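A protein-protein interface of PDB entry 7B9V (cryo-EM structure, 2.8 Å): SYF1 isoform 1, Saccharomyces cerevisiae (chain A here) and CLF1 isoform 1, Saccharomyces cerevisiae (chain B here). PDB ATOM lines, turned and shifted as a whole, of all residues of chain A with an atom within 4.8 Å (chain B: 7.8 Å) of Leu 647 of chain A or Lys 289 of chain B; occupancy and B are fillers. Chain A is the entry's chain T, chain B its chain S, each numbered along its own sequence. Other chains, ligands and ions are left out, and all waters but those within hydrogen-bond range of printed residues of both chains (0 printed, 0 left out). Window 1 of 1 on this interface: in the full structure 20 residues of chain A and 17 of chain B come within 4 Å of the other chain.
Of chain B, only Lys 289 comes within 4 Å of Leu 647 of chain A. Of the printed residues of chain A, Lys 289 of chain B touches Gln 606, Glu 609, Tyr 627, His 643 and Leu 647. Of the printed residues of chain A, Leu 285 of chain B touches Phe 646 (3.6 Å). Printed residues of chain A within 4 Å of Gly 292 of chain B: Gln 606 (3.8 Å). Of the printed residues of chain A, Asp 286 of chain B touches Lys 650. Printed residues of chain B within 4 Å of Glu 609 of chain A: Lys 289 and Gln 290. Printed residues of chain B within 4 Å of Phe 646 of chain A: Leu 285 (3.6 Å) and Ile 301 (3.4 Å). The nearest printed residue of chain A that does not touch Ile 297 of chain B is Phe 646 of chain A (6.3 Å).
The side-chain amino group of Lys 289 of chain B sits at hydrogen-bond distance from a ring nitrogen (NE2) of His 643 of chain A (3.0 Å). The side-chain hydroxyl (OH) of Tyr 627 of chain A is in hydrogen-bond range of the side-chain amino group (NZ) of Lys 289 of chain B (2.9 Å). The side-chain amino group of Lys 289 of chain B is in salt-bridge range of the side-chain carboxylate of Glu 609 of chain A (3.95 Å). The side-chain carboxylate (OD1) of Asp 286 of chain B lies within salt-bridge range of the side-chain amino group (NZ) of Lys 650 of chain A (3.0 Å).
NE2 of Gln 290 of chain B lies within hydrogen-bond range of O of Asp 286 of chain B, at 3.5 Å. OE1 of Glu 609 of chain A is in salt-bridge range of NZ of Lys 650 of chain A (3.8 Å). OE2 of Glu 609 of chain A lies within hydrogen-bond range of OH of Tyr 627 of chain A (2.7 Å).
Among the printed residues, merely in contact across the chains: Phe 646 of chain A with Ile 301 of chain B (3.4 Å), His 643 of chain A with Ile 297 of chain B (3.5 Å), Arg 645 of chain A with Arg 305 of chain B (3.6 Å), Phe 646 of chain A with Leu 285 of chain B (3.6 Å), Gln 606 of chain A with Gln 290 of chain B (3.7 Å), Gln 606 of chain A with Gly 292 of chain B (3.8 Å), Glu 609 of chain A with Gln 290 of chain B (3.8 Å), Gln 606 of chain A with Lys 289 of chain B (3.9 Å) and Leu 647 of chain A with Lys 289 of chain B (3.95 Å).
Of the 16 printed residues of chain A, 8 touch a printed residue of chain B. Of the 19 printed residues of chain B, 8 touch a printed residue of chain A. Along chain B the printed residues that touch a printed residue of chain A span positions 285 to 305. Among the printed residues, Asp or Glu carboxylates within 4 Å of a Lys or Arg side-chain nitrogen of the other chain: Glu 609 of chain A with Lys 289 of chain B and Lys 650 of chain A with Asp 286 of chain B.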
ATOM      1  N   GLN A 606     -25.009   6.010 -24.419  1.00  0.00           N
ATOM      2  CA  GLN A 606     -24.424   6.194 -23.096  1.00  0.00           C
ATOM      3  C   GLN A 606     -24.825   7.529 -22.495  1.00  0.00           C
ATOM      4  O   GLN A 606     -25.002   7.631 -21.281  1.00  0.00           O
ATOM      5  CB  GLN A 606     -22.902   6.116 -23.146  1.00  0.00           C
ATOM      6  CG  GLN A 606     -22.328   4.840 -23.709  1.00  0.00           C
ATOM      7  CD  GLN A 606     -20.814   4.861 -23.710  1.00  0.00           C
ATOM      8  OE1 GLN A 606     -20.197   5.817 -23.241  1.00  0.00           O
ATOM      9  NE2 GLN A 606     -20.207   3.813 -24.247  1.00  0.00           N
ATOM     10  N   GLU A 609     -28.324   7.201 -21.307  1.00  0.00           N
ATOM     11  CA  GLU A 609     -28.332   6.428 -20.071  1.00  0.00           C
ATOM     12  C   GLU A 609     -27.724   7.194 -18.911  1.00  0.00           C
ATOM     13  O   GLU A 609     -28.083   6.934 -17.764  1.00  0.00           O
ATOM     14  CB  GLU A 609     -27.650   5.074 -20.254  1.00  0.00           C
ATOM     15  CG  GLU A 609     -28.414   4.170 -21.218  1.00  0.00           C
ATOM     16  CD  GLU A 609     -29.702   3.541 -20.656  1.00  0.00           C
ATOM     17  OE1 GLU A 609     -30.226   3.894 -19.577  1.00  0.00           O
ATOM     18  OE2 GLU A 609     -30.286   2.735 -21.403  1.00  0.00           O
ATOM     19  N   TRP A 624     -36.835   9.689 -23.475  1.00  0.00           N
ATOM     20  CA  TRP A 624     -37.061   8.335 -23.977  1.00  0.00           C
ATOM     21  C   TRP A 624     -37.523   8.324 -25.428  1.00  0.00           C
ATOM     22  O   TRP A 624     -37.115   7.453 -26.196  1.00  0.00           O
ATOM     23  CB  TRP A 624     -38.051   7.579 -23.090  1.00  0.00           C
ATOM     24  CG  TRP A 624     -37.435   6.920 -21.863  1.00  0.00           C
ATOM     25  CD1 TRP A 624     -37.609   7.290 -20.565  1.00  0.00           C
ATOM     26  CD2 TRP A 624     -36.558   5.778 -21.838  1.00  0.00           C
ATOM     27  NE1 TRP A 624     -36.907   6.462 -19.728  1.00  0.00           N
ATOM     28  CE2 TRP A 624     -36.253   5.528 -20.484  1.00  0.00           C
ATOM     29  CE3 TRP A 624     -36.004   4.954 -22.814  1.00  0.00           C
ATOM     30  CZ2 TRP A 624     -35.416   4.483 -20.091  1.00  0.00           C
ATOM     31  CZ3 TRP A 624     -35.176   3.917 -22.422  1.00  0.00           C
ATOM     32  CH2 TRP A 624     -34.891   3.698 -21.076  1.00  0.00           C
ATOM     33  N   TYR A 627     -34.456   8.620 -27.390  1.00  0.00           N
ATOM     34  CA  TYR A 627     -33.552   7.475 -27.305  1.00  0.00           C
ATOM     35  C   TYR A 627     -34.090   6.298 -28.106  1.00  0.00           C
ATOM     36  O   TYR A 627     -33.345   5.664 -28.870  1.00  0.00           O
ATOM     37  CB  TYR A 627     -33.371   7.132 -25.819  1.00  0.00           C
ATOM     38  CG  TYR A 627     -32.477   5.975 -25.378  1.00  0.00           C
ATOM     39  CD1 TYR A 627     -31.545   5.381 -26.224  1.00  0.00           C
ATOM     40  CD2 TYR A 627     -32.547   5.535 -24.059  1.00  0.00           C
ATOM     41  CE1 TYR A 627     -30.795   4.324 -25.811  1.00  0.00           C
ATOM     42  CE2 TYR A 627     -31.755   4.503 -23.621  1.00  0.00           C
ATOM     43  CZ  TYR A 627     -30.888   3.905 -24.504  1.00  0.00           C
ATOM     44  OH  TYR A 627     -30.080   2.909 -24.066  1.00  0.00           O
ATOM     45  N   LEU A 628     -35.378   6.006 -27.967  1.00  0.00           N
ATOM     46  CA  LEU A 628     -35.981   4.899 -28.697  1.00  0.00           C
ATOM     47  C   LEU A 628     -36.036   5.169 -30.191  1.00  0.00           C
ATOM     48  O   LEU A 628     -35.782   4.254 -30.969  1.00  0.00           O
ATOM     49  CB  LEU A 628     -37.358   4.594 -28.112  1.00  0.00           C
ATOM     50  CG  LEU A 628     -37.366   4.291 -26.608  1.00  0.00           C
ATOM     51  CD1 LEU A 628     -38.648   3.696 -26.180  1.00  0.00           C
ATOM     52  CD2 LEU A 628     -36.283   3.277 -26.250  1.00  0.00           C
ATOM     53  N   ALA A 631     -32.474   4.804 -31.537  1.00  0.00           N
ATOM     54  CA  ALA A 631     -32.085   3.398 -31.479  1.00  0.00           C
ATOM     55  C   ALA A 631     -32.789   2.567 -32.547  1.00  0.00           C
ATOM     56  O   ALA A 631     -32.159   1.731 -33.205  1.00  0.00           O
ATOM     57  CB  ALA A 631     -32.390   2.848 -30.088  1.00  0.00           C
ATOM     58  N   LEU A 639     -27.641  -2.125 -32.890  1.00  0.00           N
ATOM     59  CA  LEU A 639     -28.400  -2.742 -31.810  1.00  0.00           C
ATOM     60  C   LEU A 639     -29.159  -3.968 -32.304  1.00  0.00           C
ATOM     61  O   LEU A 639     -29.948  -3.869 -33.248  1.00  0.00           O
ATOM     62  CB  LEU A 639     -29.335  -1.704 -31.188  1.00  0.00           C
ATOM     63  CG  LEU A 639     -28.807  -0.787 -30.068  1.00  0.00           C
ATOM     64  CD1 LEU A 639     -27.628   0.049 -30.410  1.00  0.00           C
ATOM     65  CD2 LEU A 639     -29.913   0.135 -29.646  1.00  0.00           C
ATOM     66  N   HIS A 643     -31.934  -6.235 -28.078  1.00  0.00           N
ATOM     67  CA  HIS A 643     -31.484  -5.058 -27.331  1.00  0.00           C
ATOM     68  C   HIS A 643     -32.515  -3.916 -27.380  1.00  0.00           C
ATOM     69  O   HIS A 643     -32.828  -3.296 -26.345  1.00  0.00           O
ATOM     70  CB  HIS A 643     -30.143  -4.597 -27.912  1.00  0.00           C
ATOM     71  CG  HIS A 643     -29.412  -3.576 -27.082  1.00  0.00           C
ATOM     72  ND1 HIS A 643     -28.156  -3.129 -27.404  1.00  0.00           N
ATOM     73  CD2 HIS A 643     -29.738  -2.964 -25.917  1.00  0.00           C
ATOM     74  CE1 HIS A 643     -27.761  -2.254 -26.508  1.00  0.00           C
ATOM     75  NE2 HIS A 643     -28.702  -2.139 -25.589  1.00  0.00           N
ATOM     76  N   ILE A 644     -33.056  -3.614 -28.565  1.00  0.00           N
ATOM     77  CA  ILE A 644     -34.140  -2.631 -28.661  1.00  0.00           C
ATOM     78  C   ILE A 644     -35.410  -3.144 -27.976  1.00  0.00           C
ATOM     79  O   ILE A 644     -36.126  -2.375 -27.296  1.00  0.00           O
ATOM     80  CB  ILE A 644     -34.370  -2.262 -30.142  1.00  0.00           C
ATOM     81  CG1 ILE A 644     -33.196  -1.462 -30.674  1.00  0.00           C
ATOM     82  CG2 ILE A 644     -35.530  -1.306 -30.307  1.00  0.00           C
ATOM     83  CD1 ILE A 644     -32.975  -1.641 -32.159  1.00  0.00           C
ATOM     84  N   ARG A 645     -35.708  -4.452 -28.132  1.00  0.00           N
ATOM     85  CA  ARG A 645     -36.844  -5.060 -27.425  1.00  0.00           C
ATOM     86  C   ARG A 645     -36.693  -5.001 -25.891  1.00  0.00           C
ATOM     87  O   ARG A 645     -37.696  -4.925 -25.169  1.00  0.00           O
ATOM     88  CB  ARG A 645     -37.066  -6.487 -27.943  1.00  0.00           C
ATOM     89  CG  ARG A 645     -38.351  -7.138 -27.460  1.00  0.00           C
ATOM     90  CD  ARG A 645     -38.534  -8.556 -27.934  1.00  0.00           C
ATOM     91  NE  ARG A 645     -38.887  -8.575 -29.350  1.00  0.00           N
ATOM     92  CZ  ARG A 645     -38.117  -9.035 -30.322  1.00  0.00           C
ATOM     93  NH1 ARG A 645     -36.969  -9.653 -30.065  1.00  0.00           N
ATOM     94  NH2 ARG A 645     -38.538  -8.932 -31.582  1.00  0.00           N
ATOM     95  N   PHE A 646     -35.453  -4.923 -25.386  1.00  0.00           N
ATOM     96  CA  PHE A 646     -35.197  -4.629 -23.974  1.00  0.00           C
ATOM     97  C   PHE A 646     -35.485  -3.181 -23.614  1.00  0.00           C
ATOM     98  O   PHE A 646     -36.047  -2.918 -22.538  1.00  0.00           O
ATOM     99  CB  PHE A 646     -33.739  -4.975 -23.641  1.00  0.00           C
ATOM    100  CG  PHE A 646     -33.208  -4.287 -22.397  1.00  0.00           C
ATOM    101  CD1 PHE A 646     -33.358  -4.877 -21.153  1.00  0.00           C
ATOM    102  CD2 PHE A 646     -32.398  -3.130 -22.495  1.00  0.00           C
ATOM    103  CE1 PHE A 646     -32.832  -4.277 -20.018  1.00  0.00           C
ATOM    104  CE2 PHE A 646     -31.844  -2.557 -21.353  1.00  0.00           C
ATOM    105  CZ  PHE A 646     -32.072  -3.131 -20.117  1.00  0.00           C
ATOM    106  N   LEU A 647     -34.956  -2.238 -24.403  1.00  0.00           N
ATOM    107  CA  LEU A 647     -35.176  -0.797 -24.176  1.00  0.00           C
ATOM    108  C   LEU A 647     -36.646  -0.428 -24.036  1.00  0.00           C
ATOM    109  O   LEU A 647     -37.022   0.364 -23.163  1.00  0.00           O
ATOM    110  CB  LEU A 647     -34.537   0.043 -25.280  1.00  0.00           C
ATOM    111  CG  LEU A 647     -33.026   0.147 -25.378  1.00  0.00           C
ATOM    112  CD1 LEU A 647     -32.637   1.141 -26.464  1.00  0.00           C
ATOM    113  CD2 LEU A 647     -32.490   0.599 -24.043  1.00  0.00           C
ATOM    114  N   PHE A 648     -37.467  -0.898 -24.967  1.00  0.00           N
ATOM    115  CA  PHE A 648     -38.904  -0.629 -24.902  1.00  0.00           C
ATOM    116  C   PHE A 648     -39.601  -1.205 -23.661  1.00  0.00           C
ATOM    117  O   PHE A 648     -40.465  -0.537 -23.092  1.00  0.00           O
ATOM    118  CB  PHE A 648     -39.582  -1.129 -26.162  1.00  0.00           C
ATOM    119  CG  PHE A 648     -39.503  -0.159 -27.304  1.00  0.00           C
ATOM    120  CD1 PHE A 648     -40.461   0.827 -27.426  1.00  0.00           C
ATOM    121  CD2 PHE A 648     -38.494  -0.231 -28.245  1.00  0.00           C
ATOM    122  CE1 PHE A 648     -40.451   1.699 -28.482  1.00  0.00           C
ATOM    123  CE2 PHE A 648     -38.455   0.664 -29.292  1.00  0.00           C
ATOM    124  CZ  PHE A 648     -39.439   1.631 -29.406  1.00  0.00           C
ATOM    125  N   GLU A 649     -39.104  -2.302 -23.095  1.00  0.00           N
ATOM    126  CA  GLU A 649     -39.630  -2.786 -21.808  1.00  0.00           C
ATOM    127  C   GLU A 649     -39.116  -2.012 -20.605  1.00  0.00           C
ATOM    128  O   GLU A 649     -39.889  -1.747 -19.671  1.00  0.00           O
ATOM    129  CB  GLU A 649     -39.300  -4.270 -21.624  1.00  0.00           C
ATOM    130  CG  GLU A 649     -39.950  -5.256 -22.605  1.00  0.00           C
ATOM    131  CD  GLU A 649     -41.481  -5.334 -22.539  1.00  0.00           C
ATOM    132  OE1 GLU A 649     -42.108  -4.880 -21.556  1.00  0.00           O
ATOM    133  OE2 GLU A 649     -42.071  -5.849 -23.511  1.00  0.00           O
ATOM    134  N   LYS A 650     -37.866  -1.560 -20.665  1.00  0.00           N
ATOM    135  CA  LYS A 650     -37.279  -0.737 -19.604  1.00  0.00           C
ATOM    136  C   LYS A 650     -37.933   0.637 -19.524  1.00  0.00           C
ATOM    137  O   LYS A 650     -38.308   1.093 -18.425  1.00  0.00           O
ATOM    138  CB  LYS A 650     -35.776  -0.587 -19.817  1.00  0.00           C
ATOM    139  CG  LYS A 650     -35.127   0.164 -18.696  1.00  0.00           C
ATOM    140  CD  LYS A 650     -33.627   0.104 -18.734  1.00  0.00           C
ATOM    141  CE  LYS A 650     -33.072   0.948 -17.606  1.00  0.00           C
ATOM    142  NZ  LYS A 650     -31.591   0.935 -17.578  1.00  0.00           N
ATOM    143  N   ALA A 651     -38.246   1.213 -20.687  1.00  0.00           N
ATOM    144  CA  ALA A 651     -38.996   2.462 -20.744  1.00  0.00           C
ATOM    145  C   ALA A 651     -40.407   2.246 -20.232  1.00  0.00           C
ATOM    146  O   ALA A 651     -40.853   3.005 -19.367  1.00  0.00           O
ATOM    147  CB  ALA A 651     -39.016   2.999 -22.177  1.00  0.00           C
ATOM    148  N   ALA B 282     -29.177  -6.764 -12.638  1.00  0.00           N
ATOM    149  CA  ALA B 282     -29.703  -5.508 -13.175  1.00  0.00           C
ATOM    150  C   ALA B 282     -28.708  -4.365 -13.020  1.00  0.00           C
ATOM    151  O   ALA B 282     -28.601  -3.499 -13.897  1.00  0.00           O
ATOM    152  CB  ALA B 282     -31.018  -5.157 -12.482  1.00  0.00           C
ATOM    153  N   GLY B 283     -28.009  -4.330 -11.876  1.00  0.00           N
ATOM    154  CA  GLY B 283     -26.990  -3.317 -11.651  1.00  0.00           C
ATOM    155  C   GLY B 283     -25.827  -3.416 -12.620  1.00  0.00           C
ATOM    156  O   GLY B 283     -25.323  -2.393 -13.106  1.00  0.00           O
ATOM    157  N   LEU B 284     -25.360  -4.655 -12.871  1.00  0.00           N
ATOM    158  CA  LEU B 284     -24.320  -4.887 -13.877  1.00  0.00           C
ATOM    159  C   LEU B 284     -24.776  -4.418 -15.243  1.00  0.00           C
ATOM    160  O   LEU B 284     -23.997  -3.816 -15.988  1.00  0.00           O
ATOM    161  CB  LEU B 284     -23.927  -6.370 -13.934  1.00  0.00           C
ATOM    162  CG  LEU B 284     -23.046  -6.876 -15.097  1.00  0.00           C
ATOM    163  CD1 LEU B 284     -21.716  -6.119 -15.236  1.00  0.00           C
ATOM    164  CD2 LEU B 284     -22.782  -8.368 -15.019  1.00  0.00           C
ATOM    165  N   LEU B 285     -26.031  -4.719 -15.593  1.00  0.00           N
ATOM    166  CA  LEU B 285     -26.563  -4.348 -16.900  1.00  0.00           C
ATOM    167  C   LEU B 285     -26.631  -2.828 -17.060  1.00  0.00           C
ATOM    168  O   LEU B 285     -26.295  -2.296 -18.122  1.00  0.00           O
ATOM    169  CB  LEU B 285     -27.918  -5.011 -17.130  1.00  0.00           C
ATOM    170  CG  LEU B 285     -28.662  -4.669 -18.405  1.00  0.00           C
ATOM    171  CD1 LEU B 285     -27.758  -4.933 -19.603  1.00  0.00           C
ATOM    172  CD2 LEU B 285     -29.833  -5.595 -18.456  1.00  0.00           C
ATOM    173  N   ASP B 286     -27.147  -2.127 -16.036  1.00  0.00           N
ATOM    174  CA  ASP B 286     -27.151  -0.657 -16.006  1.00  0.00           C
ATOM    175  C   ASP B 286     -25.752  -0.051 -16.126  1.00  0.00           C
ATOM    176  O   ASP B 286     -25.564   0.969 -16.816  1.00  0.00           O
ATOM    177  CB  ASP B 286     -27.812  -0.131 -14.727  1.00  0.00           C
ATOM    178  CG  ASP B 286     -29.284  -0.475 -14.632  1.00  0.00           C
ATOM    179  OD1 ASP B 286     -29.933  -0.634 -15.689  1.00  0.00           O
ATOM    180  OD2 ASP B 286     -29.802  -0.560 -13.497  1.00  0.00           O
ATOM    181  N   PHE B 287     -24.748  -0.695 -15.507  1.00  0.00           N
ATOM    182  CA  PHE B 287     -23.363  -0.256 -15.667  1.00  0.00           C
ATOM    183  C   PHE B 287     -22.906  -0.427 -17.101  1.00  0.00           C
ATOM    184  O   PHE B 287     -22.263   0.470 -17.664  1.00  0.00           O
ATOM    185  CB  PHE B 287     -22.438  -1.036 -14.727  1.00  0.00           C
ATOM    186  CG  PHE B 287     -20.981  -0.662 -14.859  1.00  0.00           C
ATOM    187  CD1 PHE B 287     -20.475   0.398 -14.135  1.00  0.00           C
ATOM    188  CD2 PHE B 287     -20.102  -1.418 -15.644  1.00  0.00           C
ATOM    189  CE1 PHE B 287     -19.150   0.752 -14.245  1.00  0.00           C
ATOM    190  CE2 PHE B 287     -18.777  -1.067 -15.758  1.00  0.00           C
ATOM    191  CZ  PHE B 287     -18.307   0.016 -15.053  1.00  0.00           C
ATOM    192  N   GLU B 288     -23.147  -1.602 -17.672  1.00  0.00           N
ATOM    193  CA  GLU B 288     -22.704  -1.872 -19.033  1.00  0.00           C
ATOM    194  C   GLU B 288     -23.436  -1.008 -20.049  1.00  0.00           C
ATOM    195  O   GLU B 288     -22.838  -0.645 -21.059  1.00  0.00           O
ATOM    196  CB  GLU B 288     -22.836  -3.355 -19.386  1.00  0.00           C
ATOM    197  CG  GLU B 288     -22.013  -4.338 -18.533  1.00  0.00           C
ATOM    198  CD  GLU B 288     -20.511  -4.414 -18.864  1.00  0.00           C
ATOM    199  OE1 GLU B 288     -19.796  -3.383 -18.939  1.00  0.00           O
ATOM    200  OE2 GLU B 288     -20.033  -5.555 -19.039  1.00  0.00           O
ATOM    201  N   LYS B 289     -24.703  -0.639 -19.786  1.00  0.00           N
ATOM    202  CA  LYS B 289     -25.376   0.355 -20.622  1.00  0.00           C
ATOM    203  C   LYS B 289     -24.643   1.686 -20.562  1.00  0.00           C
ATOM    204  O   LYS B 289     -24.410   2.312 -21.604  1.00  0.00           O
ATOM    205  CB  LYS B 289     -26.829   0.509 -20.179  1.00  0.00           C
ATOM    206  CG  LYS B 289     -27.690  -0.665 -20.604  1.00  0.00           C
ATOM    207  CD  LYS B 289     -27.847  -0.784 -22.101  1.00  0.00           C
ATOM    208  CE  LYS B 289     -28.607   0.358 -22.686  1.00  0.00           C
ATOM    209  NZ  LYS B 289     -28.538   0.513 -24.168  1.00  0.00           N
ATOM    210  N   GLN B 290     -24.248   2.125 -19.365  1.00  0.00           N
ATOM    211  CA  GLN B 290     -23.616   3.437 -19.276  1.00  0.00           C
ATOM    212  C   GLN B 290     -22.150   3.444 -19.725  1.00  0.00           C
ATOM    213  O   GLN B 290     -21.643   4.508 -20.100  1.00  0.00           O
ATOM    214  CB  GLN B 290     -23.734   3.984 -17.858  1.00  0.00           C
ATOM    215  CG  GLN B 290     -25.126   4.425 -17.478  1.00  0.00           C
ATOM    216  CD  GLN B 290     -25.206   4.807 -16.026  1.00  0.00           C
ATOM    217  OE1 GLN B 290     -24.586   5.776 -15.592  1.00  0.00           O
ATOM    218  NE2 GLN B 290     -25.970   4.044 -15.258  1.00  0.00           N
ATOM    219  N   PHE B 291     -21.447   2.300 -19.691  1.00  0.00           N
ATOM    220  CA  PHE B 291     -20.015   2.262 -20.001  1.00  0.00           C
ATOM    221  C   PHE B 291     -19.670   0.989 -20.764  1.00  0.00           C
ATOM    222  O   PHE B 291     -20.152  -0.092 -20.433  1.00  0.00           O
ATOM    223  CB  PHE B 291     -19.112   2.313 -18.746  1.00  0.00           C
ATOM    224  CG  PHE B 291     -19.392   3.471 -17.818  1.00  0.00           C
ATOM    225  CD1 PHE B 291     -20.356   3.379 -16.824  1.00  0.00           C
ATOM    226  CD2 PHE B 291     -18.725   4.672 -17.985  1.00  0.00           C
ATOM    227  CE1 PHE B 291     -20.623   4.453 -15.984  1.00  0.00           C
ATOM    228  CE2 PHE B 291     -18.985   5.752 -17.156  1.00  0.00           C
ATOM    229  CZ  PHE B 291     -19.934   5.642 -16.155  1.00  0.00           C
ATOM    230  N   GLY B 292     -18.666   1.081 -21.632  1.00  0.00           N
ATOM    231  CA  GLY B 292     -18.128  -0.107 -22.264  1.00  0.00           C
ATOM    232  C   GLY B 292     -18.756  -0.386 -23.622  1.00  0.00           C
ATOM    233  O   GLY B 292     -19.853   0.066 -23.943  1.00  0.00           O
ATOM    234  N   ASP B 293     -18.036  -1.174 -24.425  1.00  0.00           N
ATOM    235  CA  ASP B 293     -18.383  -1.470 -25.816  1.00  0.00           C
ATOM    236  C   ASP B 293     -19.592  -2.403 -25.915  1.00  0.00           C
ATOM    237  O   ASP B 293     -19.918  -3.128 -24.972  1.00  0.00           O
ATOM    238  CB  ASP B 293     -17.185  -2.088 -26.535  1.00  0.00           C
ATOM    239  CG  ASP B 293     -16.045  -1.110 -26.705  1.00  0.00           C
ATOM    240  OD1 ASP B 293     -16.244   0.090 -26.420  1.00  0.00           O
ATOM    241  OD2 ASP B 293     -14.959  -1.538 -27.140  1.00  0.00           O
ATOM    242  N   ILE B 294     -20.235  -2.381 -27.103  1.00  0.00           N
ATOM    243  CA  ILE B 294     -21.580  -2.937 -27.314  1.00  0.00           C
ATOM    244  C   ILE B 294     -21.666  -4.444 -27.071  1.00  0.00           C
ATOM    245  O   ILE B 294     -22.718  -4.918 -26.611  1.00  0.00           O
ATOM    246  CB  ILE B 294     -22.104  -2.584 -28.743  1.00  0.00           C
ATOM    247  CG1 ILE B 294     -23.615  -2.885 -28.906  1.00  0.00           C
ATOM    248  CG2 ILE B 294     -21.238  -3.169 -29.902  1.00  0.00           C
ATOM    249  CD1 ILE B 294     -24.205  -2.547 -30.255  1.00  0.00           C
ATOM    250  N   SER B 296     -20.438  -6.459 -24.846  1.00  0.00           N
ATOM    251  CA  SER B 296     -20.753  -6.770 -23.459  1.00  0.00           C
ATOM    252  C   SER B 296     -22.236  -6.593 -23.189  1.00  0.00           C
ATOM    253  O   SER B 296     -22.856  -7.427 -22.510  1.00  0.00           O
ATOM    254  CB  SER B 296     -19.922  -5.887 -22.534  1.00  0.00           C
ATOM    255  OG  SER B 296     -20.219  -4.512 -22.728  1.00  0.00           O
ATOM    256  N   ILE B 297     -22.805  -5.485 -23.691  1.00  0.00           N
ATOM    257  CA  ILE B 297     -24.222  -5.226 -23.492  1.00  0.00           C
ATOM    258  C   ILE B 297     -25.067  -6.266 -24.189  1.00  0.00           C
ATOM    259  O   ILE B 297     -26.005  -6.782 -23.598  1.00  0.00           O
ATOM    260  CB  ILE B 297     -24.609  -3.816 -23.969  1.00  0.00           C
ATOM    261  CG1 ILE B 297     -23.843  -2.774 -23.217  1.00  0.00           C
ATOM    262  CG2 ILE B 297     -26.057  -3.543 -23.705  1.00  0.00           C
ATOM    263  CD1 ILE B 297     -22.868  -2.052 -23.998  1.00  0.00           C
ATOM    264  N   GLU B 298     -24.659  -6.678 -25.404  1.00  0.00           N
ATOM    265  CA  GLU B 298     -25.430  -7.661 -26.166  1.00  0.00           C
ATOM    266  C   GLU B 298     -25.470  -9.001 -25.447  1.00  0.00           C
ATOM    267  O   GLU B 298     -26.536  -9.622 -25.341  1.00  0.00           O
ATOM    268  CB  GLU B 298     -24.858  -7.795 -27.573  1.00  0.00           C
ATOM    269  CG  GLU B 298     -25.826  -8.419 -28.579  1.00  0.00           C
ATOM    270  CD  GLU B 298     -25.618  -9.903 -28.784  1.00  0.00           C
ATOM    271  OE1 GLU B 298     -24.451 -10.330 -28.894  1.00  0.00           O
ATOM    272  OE2 GLU B 298     -26.623 -10.642 -28.848  1.00  0.00           O
ATOM    273  N   THR B 300     -24.904  -9.557 -22.141  1.00  0.00           N
ATOM    274  CA  THR B 300     -25.595  -9.390 -20.862  1.00  0.00           C
ATOM    275  C   THR B 300     -27.105  -9.333 -21.047  1.00  0.00           C
ATOM    276  O   THR B 300     -27.870  -9.940 -20.270  1.00  0.00           O
ATOM    277  CB  THR B 300     -25.092  -8.134 -20.152  1.00  0.00           C
ATOM    278  OG1 THR B 300     -23.660  -8.101 -20.186  1.00  0.00           O
ATOM    279  CG2 THR B 300     -25.541  -8.128 -18.695  1.00  0.00           C
ATOM    280  N   ILE B 301     -27.541  -8.597 -22.083  1.00  0.00           N
ATOM    281  CA  ILE B 301     -28.946  -8.524 -22.449  1.00  0.00           C
ATOM    282  C   ILE B 301     -29.463  -9.886 -22.821  1.00  0.00           C
ATOM    283  O   ILE B 301     -30.576 -10.246 -22.434  1.00  0.00           O
ATOM    284  CB  ILE B 301     -29.156  -7.512 -23.600  1.00  0.00           C
ATOM    285  CG1 ILE B 301     -29.017  -6.132 -22.999  1.00  0.00           C
ATOM    286  CG2 ILE B 301     -30.472  -7.738 -24.447  1.00  0.00           C
ATOM    287  CD1 ILE B 301     -30.116  -5.783 -22.302  1.00  0.00           C
ATOM    288  N   ARG B 305     -32.637 -11.540 -21.027  1.00  0.00           N
ATOM    289  CA  ARG B 305     -33.813 -11.847 -21.833  1.00  0.00           C
ATOM    290  C   ARG B 305     -34.104 -13.339 -21.847  1.00  0.00           C
ATOM    291  O   ARG B 305     -35.276 -13.721 -21.860  1.00  0.00           O
ATOM    292  CB  ARG B 305     -33.644 -11.281 -23.246  1.00  0.00           C
ATOM    293  CG  ARG B 305     -33.584  -9.740 -23.314  1.00  0.00           C
ATOM    294  CD  ARG B 305     -34.850  -9.038 -22.900  1.00  0.00           C
ATOM    295  NE  ARG B 305     -35.922  -9.378 -23.833  1.00  0.00           N
ATOM    296  CZ  ARG B 305     -37.213  -9.208 -23.600  1.00  0.00           C
ATOM    297  NH1 ARG B 305     -37.642  -8.578 -22.514  1.00  0.00           N
ATOM    298  NH2 ARG B 305     -38.093  -9.624 -24.508  1.00  0.00           N
